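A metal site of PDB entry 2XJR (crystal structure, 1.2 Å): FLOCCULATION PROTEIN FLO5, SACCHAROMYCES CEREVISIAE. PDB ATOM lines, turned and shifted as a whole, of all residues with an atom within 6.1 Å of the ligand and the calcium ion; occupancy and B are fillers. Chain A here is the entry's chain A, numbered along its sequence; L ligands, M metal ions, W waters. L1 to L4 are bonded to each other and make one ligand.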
ATOM      1  N   LYS A  36      -7.450 -22.244  21.677  1.00  0.00           N
ATOM      2  CA  LYS A  36      -6.704 -21.426  20.714  1.00  0.00           C
ATOM      3  C   LYS A  36      -5.278 -21.087  21.133  1.00  0.00           C
ATOM      4  O   LYS A  36      -4.635 -20.244  20.521  1.00  0.00           O
ATOM      5  CB  LYS A  36      -7.516 -20.240  20.247  1.00  0.00           C
ATOM      6  CG  LYS A  36      -8.682 -20.675  19.348  1.00  0.00           C
ATOM      7  CD  LYS A  36      -9.679 -19.596  18.994  1.00  0.00           C
ATOM      8  CE  LYS A  36     -10.310 -18.984  20.205  1.00  0.00           C
ATOM      9  NZ  LYS A  36     -11.461 -18.135  19.827  1.00  0.00           N
ATOM     10  N   TYR A  41       1.653 -26.473  23.116  1.00  0.00           N
ATOM     11  CA  TYR A  41       1.787 -27.842  22.633  1.00  0.00           C
ATOM     12  C   TYR A  41       2.920 -28.066  21.644  1.00  0.00           C
ATOM     13  O   TYR A  41       3.117 -29.172  21.150  1.00  0.00           O
ATOM     14  CB  TYR A  41       0.453 -28.292  22.006  1.00  0.00           C
ATOM     15  CG  TYR A  41      -0.175 -27.576  20.831  1.00  0.00           C
ATOM     16  CD1 TYR A  41      -1.534 -27.694  20.560  1.00  0.00           C
ATOM     17  CD2 TYR A  41       0.573 -26.744  19.988  1.00  0.00           C
ATOM     18  CE1 TYR A  41      -2.117 -27.062  19.492  1.00  0.00           C
ATOM     19  CE2 TYR A  41      -0.027 -26.074  18.907  1.00  0.00           C
ATOM     20  CZ  TYR A  41      -1.363 -26.281  18.634  1.00  0.00           C
ATOM     21  OH  TYR A  41      -1.941 -25.617  17.563  1.00  0.00           O
ATOM     22  N   ILE A  72     -16.506 -31.317  15.544  1.00  0.00           N
ATOM     23  CA  ILE A  72     -17.329 -30.294  16.153  1.00  0.00           C
ATOM     24  C   ILE A  72     -18.762 -30.368  15.650  1.00  0.00           C
ATOM     25  O   ILE A  72     -19.047 -30.864  14.558  1.00  0.00           O
ATOM     26  CB  ILE A  72     -16.767 -28.886  15.953  1.00  0.00           C
ATOM     27  CG1 ILE A  72     -16.569 -28.504  14.494  1.00  0.00           C
ATOM     28  CG2 ILE A  72     -15.515 -28.667  16.810  1.00  0.00           C
ATOM     29  CD1 ILE A  72     -16.443 -26.995  14.254  1.00  0.00           C
ATOM     30  N   GLN A  85     -14.665 -33.185   9.225  1.00  0.00           N
ATOM     31  CA  GLN A  85     -13.962 -32.001   8.755  1.00  0.00           C
ATOM     32  C   GLN A  85     -13.961 -31.859   7.237  1.00  0.00           C
ATOM     33  O   GLN A  85     -14.057 -30.765   6.698  1.00  0.00           O
ATOM     34  CB  GLN A  85     -12.534 -31.969   9.335  1.00  0.00           C
ATOM     35  CG  GLN A  85     -11.876 -30.597   9.140  1.00  0.00           C
ATOM     36  CD  GLN A  85     -10.543 -30.410   9.872  1.00  0.00           C
ATOM     37  OE1 GLN A  85      -9.986 -29.318   9.855  1.00  0.00           O
ATOM     38  NE2 GLN A  85     -10.020 -31.464  10.453  1.00  0.00           N
ATOM     39  N   GLY A  90     -17.332 -23.571   2.971  1.00  0.00           N
ATOM     40  CA  GLY A  90     -17.825 -22.208   3.086  1.00  0.00           C
ATOM     41  C   GLY A  90     -17.475 -21.593   4.430  1.00  0.00           C
ATOM     42  O   GLY A  90     -16.421 -21.851   5.025  1.00  0.00           O
ATOM     43  N   ASN A  91     -18.360 -20.736   4.915  1.00  0.00           N
ATOM     44  CA  ASN A  91     -18.118 -19.980   6.119  1.00  0.00           C
ATOM     45  C   ASN A  91     -19.247 -19.965   7.145  1.00  0.00           C
ATOM     46  O   ASN A  91     -19.639 -18.883   7.601  1.00  0.00           O
ATOM     47  CB  ASN A  91     -17.775 -18.546   5.735  1.00  0.00           C
ATOM     48  CG  ASN A  91     -16.856 -17.922   6.746  1.00  0.00           C
ATOM     49  OD1 ASN A  91     -16.391 -18.535   7.701  1.00  0.00           O
ATOM     50  ND2 ASN A  91     -16.602 -16.656   6.524  1.00  0.00           N
ATOM     51  N   GLN A 104     -16.882 -22.035  14.766  1.00  0.00           N
ATOM     52  CA  GLN A 104     -15.797 -22.981  14.830  1.00  0.00           C
ATOM     53  C   GLN A 104     -14.743 -22.638  15.873  1.00  0.00           C
ATOM     54  O   GLN A 104     -13.828 -23.435  16.128  1.00  0.00           O
ATOM     55  CB  GLN A 104     -15.083 -23.127  13.489  1.00  0.00           C
ATOM     56  CG  GLN A 104     -15.926 -23.660  12.367  1.00  0.00           C
ATOM     57  CD  GLN A 104     -15.068 -24.015  11.140  1.00  0.00           C
ATOM     58  OE1 GLN A 104     -13.841 -24.107  11.179  1.00  0.00           O
ATOM     59  NE2 GLN A 104     -15.749 -24.366  10.059  1.00  0.00           N
ATOM     60  N   GLY A 105     -14.825 -21.461  16.478  1.00  0.00           N
ATOM     61  CA  GLY A 105     -13.807 -20.939  17.350  1.00  0.00           C
ATOM     62  C   GLY A 105     -14.078 -20.911  18.844  1.00  0.00           C
ATOM     63  O   GLY A 105     -13.312 -20.313  19.570  1.00  0.00           O
ATOM     64  N   ILE A 106     -15.164 -21.555  19.302  1.00  0.00           N
ATOM     65  CA  ILE A 106     -15.482 -21.647  20.695  1.00  0.00           C
ATOM     66  C   ILE A 106     -15.219 -23.074  21.219  1.00  0.00           C
ATOM     67  O   ILE A 106     -15.039 -24.011  20.442  1.00  0.00           O
ATOM     68  CB  ILE A 106     -16.942 -21.219  20.970  1.00  0.00           C
ATOM     69  CG1 ILE A 106     -17.990 -22.137  20.325  1.00  0.00           C
ATOM     70  CG2 ILE A 106     -17.142 -19.721  20.633  1.00  0.00           C
ATOM     71  CD1 ILE A 106     -19.417 -21.866  20.780  1.00  0.00           C
ATOM     72  N   THR A 121     -12.404 -29.886  22.065  1.00  0.00           N
ATOM     73  CA  THR A 121     -11.795 -28.767  21.330  1.00  0.00           C
ATOM     74  C   THR A 121     -10.492 -28.286  21.905  1.00  0.00           C
ATOM     75  O   THR A 121      -9.695 -27.696  21.189  1.00  0.00           O
ATOM     76  CB  THR A 121     -12.793 -27.573  21.357  1.00  0.00           C
ATOM     77  OG1 THR A 121     -13.297 -27.346  22.676  1.00  0.00           O
ATOM     78  CG2 THR A 121     -13.953 -27.799  20.410  1.00  0.00           C
ATOM     79  N   ASP A 147      -3.833 -33.896  14.681  1.00  0.00           N
ATOM     80  CA  ASP A 147      -4.479 -32.586  14.809  1.00  0.00           C
ATOM     81  C   ASP A 147      -4.878 -32.468  16.283  1.00  0.00           C
ATOM     82  O   ASP A 147      -5.851 -33.150  16.695  1.00  0.00           O
ATOM     83  CB  ASP A 147      -5.700 -32.491  13.897  1.00  0.00           C
ATOM     84  CG  ASP A 147      -6.442 -31.155  14.021  1.00  0.00           C
ATOM     85  OD1 ASP A 147      -6.281 -30.484  15.042  1.00  0.00           O
ATOM     86  OD2 ASP A 147      -7.265 -30.835  13.130  1.00  0.00           O
ATOM     87  N   ASP A 148      -4.122 -31.754  17.137  1.00  0.00           N
ATOM     88  CA  ASP A 148      -3.080 -30.790  16.783  1.00  0.00           C
ATOM     89  C   ASP A 148      -1.646 -31.281  17.056  1.00  0.00           C
ATOM     90  O   ASP A 148      -0.759 -30.961  16.265  1.00  0.00           O
ATOM     91  CB  ASP A 148      -3.315 -29.476  17.538  1.00  0.00           C
ATOM     92  CG  ASP A 148      -4.397 -28.628  16.888  1.00  0.00           C
ATOM     93  OD1 ASP A 148      -4.125 -28.101  15.788  1.00  0.00           O
ATOM     94  OD2 ASP A 148      -5.481 -28.525  17.462  1.00  0.00           O
ATOM     95  N   LYS A 181       3.477 -30.414  17.120  1.00  0.00           N
ATOM     96  CA  LYS A 181       3.144 -29.400  16.119  1.00  0.00           C
ATOM     97  C   LYS A 181       4.335 -28.450  15.965  1.00  0.00           C
ATOM     98  O   LYS A 181       4.752 -27.836  16.937  1.00  0.00           O
ATOM     99  CB  LYS A 181       1.852 -28.697  16.514  1.00  0.00           C
ATOM    100  CG  LYS A 181       1.403 -27.590  15.584  1.00  0.00           C
ATOM    101  CD  LYS A 181       1.277 -27.987  14.159  1.00  0.00           C
ATOM    102  CE  LYS A 181      -0.125 -28.091  13.626  1.00  0.00           C
ATOM    103  NZ  LYS A 181      -0.144 -29.021  12.472  1.00  0.00           N
ATOM    104  N   TYR A 209      -1.533 -36.382  23.731  1.00  0.00           N
ATOM    105  CA  TYR A 209      -2.258 -35.786  22.622  1.00  0.00           C
ATOM    106  C   TYR A 209      -2.867 -34.464  23.069  1.00  0.00           C
ATOM    107  O   TYR A 209      -3.447 -34.397  24.164  1.00  0.00           O
ATOM    108  CB  TYR A 209      -3.421 -36.754  22.229  1.00  0.00           C
ATOM    109  CG  TYR A 209      -4.438 -36.066  21.330  1.00  0.00           C
ATOM    110  CD1 TYR A 209      -4.163 -35.830  20.004  1.00  0.00           C
ATOM    111  CD2 TYR A 209      -5.601 -35.524  21.844  1.00  0.00           C
ATOM    112  CE1 TYR A 209      -5.013 -35.084  19.213  1.00  0.00           C
ATOM    113  CE2 TYR A 209      -6.453 -34.769  21.052  1.00  0.00           C
ATOM    114  CZ  TYR A 209      -6.163 -34.559  19.738  1.00  0.00           C
ATOM    115  OH  TYR A 209      -7.029 -33.789  19.006  1.00  0.00           O
ATOM    116  N   ASN A 211      -5.321 -31.036  21.625  1.00  0.00           N
ATOM    117  CA  ASN A 211      -6.149 -30.260  20.716  1.00  0.00           C
ATOM    118  C   ASN A 211      -6.271 -28.841  21.263  1.00  0.00           C
ATOM    119  O   ASN A 211      -6.515 -28.691  22.454  1.00  0.00           O
ATOM    120  CB  ASN A 211      -7.527 -30.879  20.542  1.00  0.00           C
ATOM    121  CG  ASN A 211      -8.277 -30.339  19.332  1.00  0.00           C
ATOM    122  OD1 ASN A 211      -7.644 -29.732  18.448  1.00  0.00           O
ATOM    123  ND2 ASN A 211      -9.585 -30.568  19.262  1.00  0.00           N
ATOM    124  N   ALA A 212      -6.118 -27.837  20.407  1.00  0.00           N
ATOM    125  CA  ALA A 212      -6.290 -26.447  20.770  1.00  0.00           C
ATOM    126  C   ALA A 212      -7.576 -25.827  20.263  1.00  0.00           C
ATOM    127  O   ALA A 212      -8.054 -24.826  20.839  1.00  0.00           O
ATOM    128  CB  ALA A 212      -5.143 -25.566  20.254  1.00  0.00           C
ATOM    129  N   VAL A 213      -8.125 -26.333  19.168  1.00  0.00           N
ATOM    130  CA  VAL A 213      -9.339 -25.758  18.619  1.00  0.00           C
ATOM    131  C   VAL A 213     -10.015 -26.779  17.726  1.00  0.00           C
ATOM    132  O   VAL A 213      -9.343 -27.612  17.108  1.00  0.00           O
ATOM    133  CB  VAL A 213      -9.083 -24.437  17.893  1.00  0.00           C
ATOM    134  CG1 VAL A 213      -8.284 -24.682  16.638  1.00  0.00           C
ATOM    135  CG2 VAL A 213     -10.354 -23.622  17.653  1.00  0.00           C
ATOM    136  N   SER A 214     -11.324 -26.677  17.613  1.00  0.00           N
ATOM    137  CA  SER A 214     -12.154 -27.407  16.719  1.00  0.00           C
ATOM    138  C   SER A 214     -11.802 -28.911  16.626  1.00  0.00           C
ATOM    139  O   SER A 214     -11.838 -29.594  17.641  1.00  0.00           O
ATOM    140  CB  SER A 214     -12.355 -26.674  15.387  1.00  0.00           C
ATOM    141  OG  SER A 214     -11.145 -26.584  14.643  1.00  0.00           O
ATOM    142  N   TRP A 215     -11.601 -29.415  15.424  1.00  0.00           N
ATOM    143  CA  TRP A 215     -11.416 -30.859  15.199  1.00  0.00           C
ATOM    144  C   TRP A 215     -10.194 -31.413  15.917  1.00  0.00           C
ATOM    145  O   TRP A 215      -9.187 -30.748  16.103  1.00  0.00           O
ATOM    146  CB  TRP A 215     -11.346 -31.122  13.695  1.00  0.00           C
ATOM    147  CG  TRP A 215     -12.653 -30.967  12.987  1.00  0.00           C
ATOM    148  CD1 TRP A 215     -13.545 -31.963  12.782  1.00  0.00           C
ATOM    149  CD2 TRP A 215     -13.229 -29.795  12.346  1.00  0.00           C
ATOM    150  NE1 TRP A 215     -14.671 -31.506  12.148  1.00  0.00           N
ATOM    151  CE2 TRP A 215     -14.497 -30.180  11.846  1.00  0.00           C
ATOM    152  CE3 TRP A 215     -12.812 -28.476  12.192  1.00  0.00           C
ATOM    153  CZ2 TRP A 215     -15.330 -29.294  11.187  1.00  0.00           C
ATOM    154  CZ3 TRP A 215     -13.668 -27.608  11.497  1.00  0.00           C
ATOM    155  CH2 TRP A 215     -14.866 -28.042  11.007  1.00  0.00           C
ATOM    156  N   GLY A 216     -10.297 -32.678  16.295  1.00  0.00           N
ATOM    157  CA  GLY A 216      -9.185 -33.404  16.915  1.00  0.00           C
ATOM    158  C   GLY A 216      -9.071 -34.749  16.218  1.00  0.00           C
ATOM    159  O   GLY A 216     -10.054 -35.465  16.087  1.00  0.00           O
HETATM  160  C1  LIG L   1      -8.385 -25.710  11.724  1.00  0.00           C
HETATM  161  C2  LIG L   1      -8.728 -27.157  12.090  1.00  0.00           C
HETATM  162  C3  LIG L   1      -8.327 -27.385  13.559  1.00  0.00           C
HETATM  163  C4  LIG L   1      -6.822 -27.070  13.749  1.00  0.00           C
HETATM  164  C5  LIG L   1      -6.564 -25.619  13.270  1.00  0.00           C
HETATM  165  C6  LIG L   1      -5.126 -25.156  13.428  1.00  0.00           C
HETATM  166  O1  LIG L   1      -8.035 -28.092  11.270  1.00  0.00           O
HETATM  167  O2  LIG L   1      -8.640 -28.673  14.022  1.00  0.00           O
HETATM  168  O3  LIG L   1      -6.531 -27.173  15.122  1.00  0.00           O
HETATM  169  O4  LIG L   1      -7.005 -25.445  11.924  1.00  0.00           O
HETATM  170  O5  LIG L   1      -4.322 -25.954  12.589  1.00  0.00           O
HETATM  171  C1  LG2 L   2      -8.724 -22.602  11.758  1.00  0.00           C
HETATM  172  C2  LG2 L   2      -9.752 -23.735  11.869  1.00  0.00           C
HETATM  173  C3  LG2 L   2     -10.956 -23.333  12.730  1.00  0.00           C
HETATM  174  C4  LG2 L   2     -10.518 -22.658  14.026  1.00  0.00           C
HETATM  175  C5  LG2 L   2      -9.514 -21.545  13.779  1.00  0.00           C
HETATM  176  C6  LG2 L   2      -8.916 -20.998  15.076  1.00  0.00           C
HETATM  177  O1  LG2 L   2      -9.190 -24.855  12.536  1.00  0.00           O
HETATM  178  O2  LG2 L   2     -11.821 -24.426  12.971  1.00  0.00           O
HETATM  179  O3  LG2 L   2     -11.622 -22.108  14.706  1.00  0.00           O
HETATM  180  O4  LG2 L   2      -8.421 -22.073  13.037  1.00  0.00           O
HETATM  181  O5  LG2 L   2      -8.242 -19.782  14.828  1.00  0.00           O
HETATM  182  C1  LG3 L   3      -7.715 -18.277  10.300  1.00  0.00           C
HETATM  183  C2  LG3 L   3      -8.606 -19.312  10.992  1.00  0.00           C
HETATM  184  C3  LG3 L   3      -8.364 -20.713  10.441  1.00  0.00           C
HETATM  185  C4  LG3 L   3      -8.519 -20.615   8.924  1.00  0.00           C
HETATM  186  C5  LG3 L   3      -7.609 -19.519   8.384  1.00  0.00           C
HETATM  187  C6  LG3 L   3      -7.605 -19.551   6.857  1.00  0.00           C
HETATM  188  O1  LG3 L   3      -6.469 -18.336  10.951  1.00  0.00           O
HETATM  189  O2  LG3 L   3      -9.938 -19.038  10.636  1.00  0.00           O
HETATM  190  O3  LG3 L   3      -9.330 -21.646  10.874  1.00  0.00           O
HETATM  191  O4  LG3 L   3      -8.199 -21.839   8.301  1.00  0.00           O
HETATM  192  O5  LG3 L   3      -8.052 -18.283   8.926  1.00  0.00           O
HETATM  193  O6  LG3 L   3      -8.830 -19.039   6.398  1.00  0.00           O
HETATM  194  C1  LG4 L   4      -8.794 -19.016   4.952  1.00  0.00           C
HETATM  195  C2  LG4 L   4      -9.928 -18.156   4.388  1.00  0.00           C
HETATM  196  C3  LG4 L   4     -11.286 -18.764   4.727  1.00  0.00           C
HETATM  197  C4  LG4 L   4     -11.294 -20.264   4.437  1.00  0.00           C
HETATM  198  C5  LG4 L   4     -10.044 -20.957   4.978  1.00  0.00           C
HETATM  199  C6  LG4 L   4     -10.016 -22.433   4.590  1.00  0.00           C
HETATM  200  O1  LG4 L   4      -9.766 -18.036   2.997  1.00  0.00           O
HETATM  201  O2  LG4 L   4     -12.309 -18.097   4.014  1.00  0.00           O
HETATM  202  O3  LG4 L   4     -12.432 -20.849   5.035  1.00  0.00           O
HETATM  203  O4  LG4 L   4      -8.893 -20.331   4.455  1.00  0.00           O
HETATM  204  O5  LG4 L   4      -9.722 -22.514   3.223  1.00  0.00           O
HETATM  205 CA    CA M   1      -7.646 -29.021  16.217  1.00  0.00          CA
HETATM  206  O   HOH W   1      -4.503 -25.206  16.858  1.00  0.00           O
HETATM  207  O   HOH W   2     -10.578 -23.101   7.857  1.00  0.00           O
HETATM  208  O   HOH W   3      -2.372 -26.733  14.448  1.00  0.00           O
HETATM  209  O   HOH W   4     -12.637 -19.526  14.259  1.00  0.00           O
HETATM  210  O   HOH W   5     -12.319 -20.059  10.698  1.00  0.00           O
HETATM  211  O   HOH W   6      -6.669 -18.618  16.746  1.00  0.00           O
HETATM  212  O   HOH W   7      -5.066 -29.407  11.088  1.00  0.00           O
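Water W3 lies within hydrogen-bond range of OD1 of Asp 148, O5 of LIG L1 and OH of Tyr 41.
Water W7 lies within hydrogen-bond range of an oxygen (O1) of LIG L1 (3.3 Å) and the side-chain carboxylate of Asp 147 (3.3 Å).
Water W1 bridges OH of Tyr 41 and OD1 of Asp 148.
The backbone carbonyl oxygen (O) of Asp 147 lies within hydrogen-bond range of the side-chain hydroxyl (OH) of Tyr 209 (2.7 Å).
O of Thr 121 lies within hydrogen-bond range of ND2 of Asn 211 (3.5 Å).
N of Val 213 sits at hydrogen-bond distance from O of Thr 121, at 2.9 Å.
The backbone carbonyl oxygen of Gly 105 is in hydrogen-bond range of the side-chain amino group of Lys 36, 2.9 Å away.
ND2 of Asn 211 is in hydrogen-bond range of O of Ser 214 (2.9 Å).
The side-chain carboxylate of Asp 148 sits close to the backbone NH of Ala 212 (3.1 Å).
The calcium ion is bound by the backbone carbonyl oxygen (O) of Trp 215 (2.3 Å), the side-chain carboxylate (OD1) of Asp 147 (2.3 Å), the side-chain amide oxygen (OD1) of Asn 211 (2.3 Å), the backbone carbonyl oxygen (O) of Val 213 (2.4 Å), an oxygen (O3) of LIG L1 (2.4 Å), an oxygen (O2) of LIG L1 (2.4 Å) and the side-chain carboxylate (OD2) of Asp 148 (2.5 Å).
The calcium ion has seven donor atoms within binding distance.
Within 4 Å of the calcium ion: Asp 147, Asp 148, Asn 211, Val 213 and Trp 215.
CA of Gly 105 touches O3 of LG2 L2 (3.6 Å).
Hydrophobic or aromatic side chains that line the ligand: Val 213 and Trp 215.
The side-chain amide oxygen (OE1) of Gln 85 sits at hydrogen-bond distance from an oxygen (O1) of LIG L1 (2.7 Å).
The side-chain hydroxyl (OG) of Ser 214 lies within hydrogen-bond range of an oxygen (O2) of LG2 L2.
The backbone NH of Trp 215 lies close to an oxygen (O2) of LIG L1 (3.4 Å).
O2 of LG2 L2 sits at hydrogen-bond distance from OE1 of Gln 104, at 2.7 Å.
O3 of LG2 L2 lies within hydrogen-bond range of O of Gln 104 (2.9 Å).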
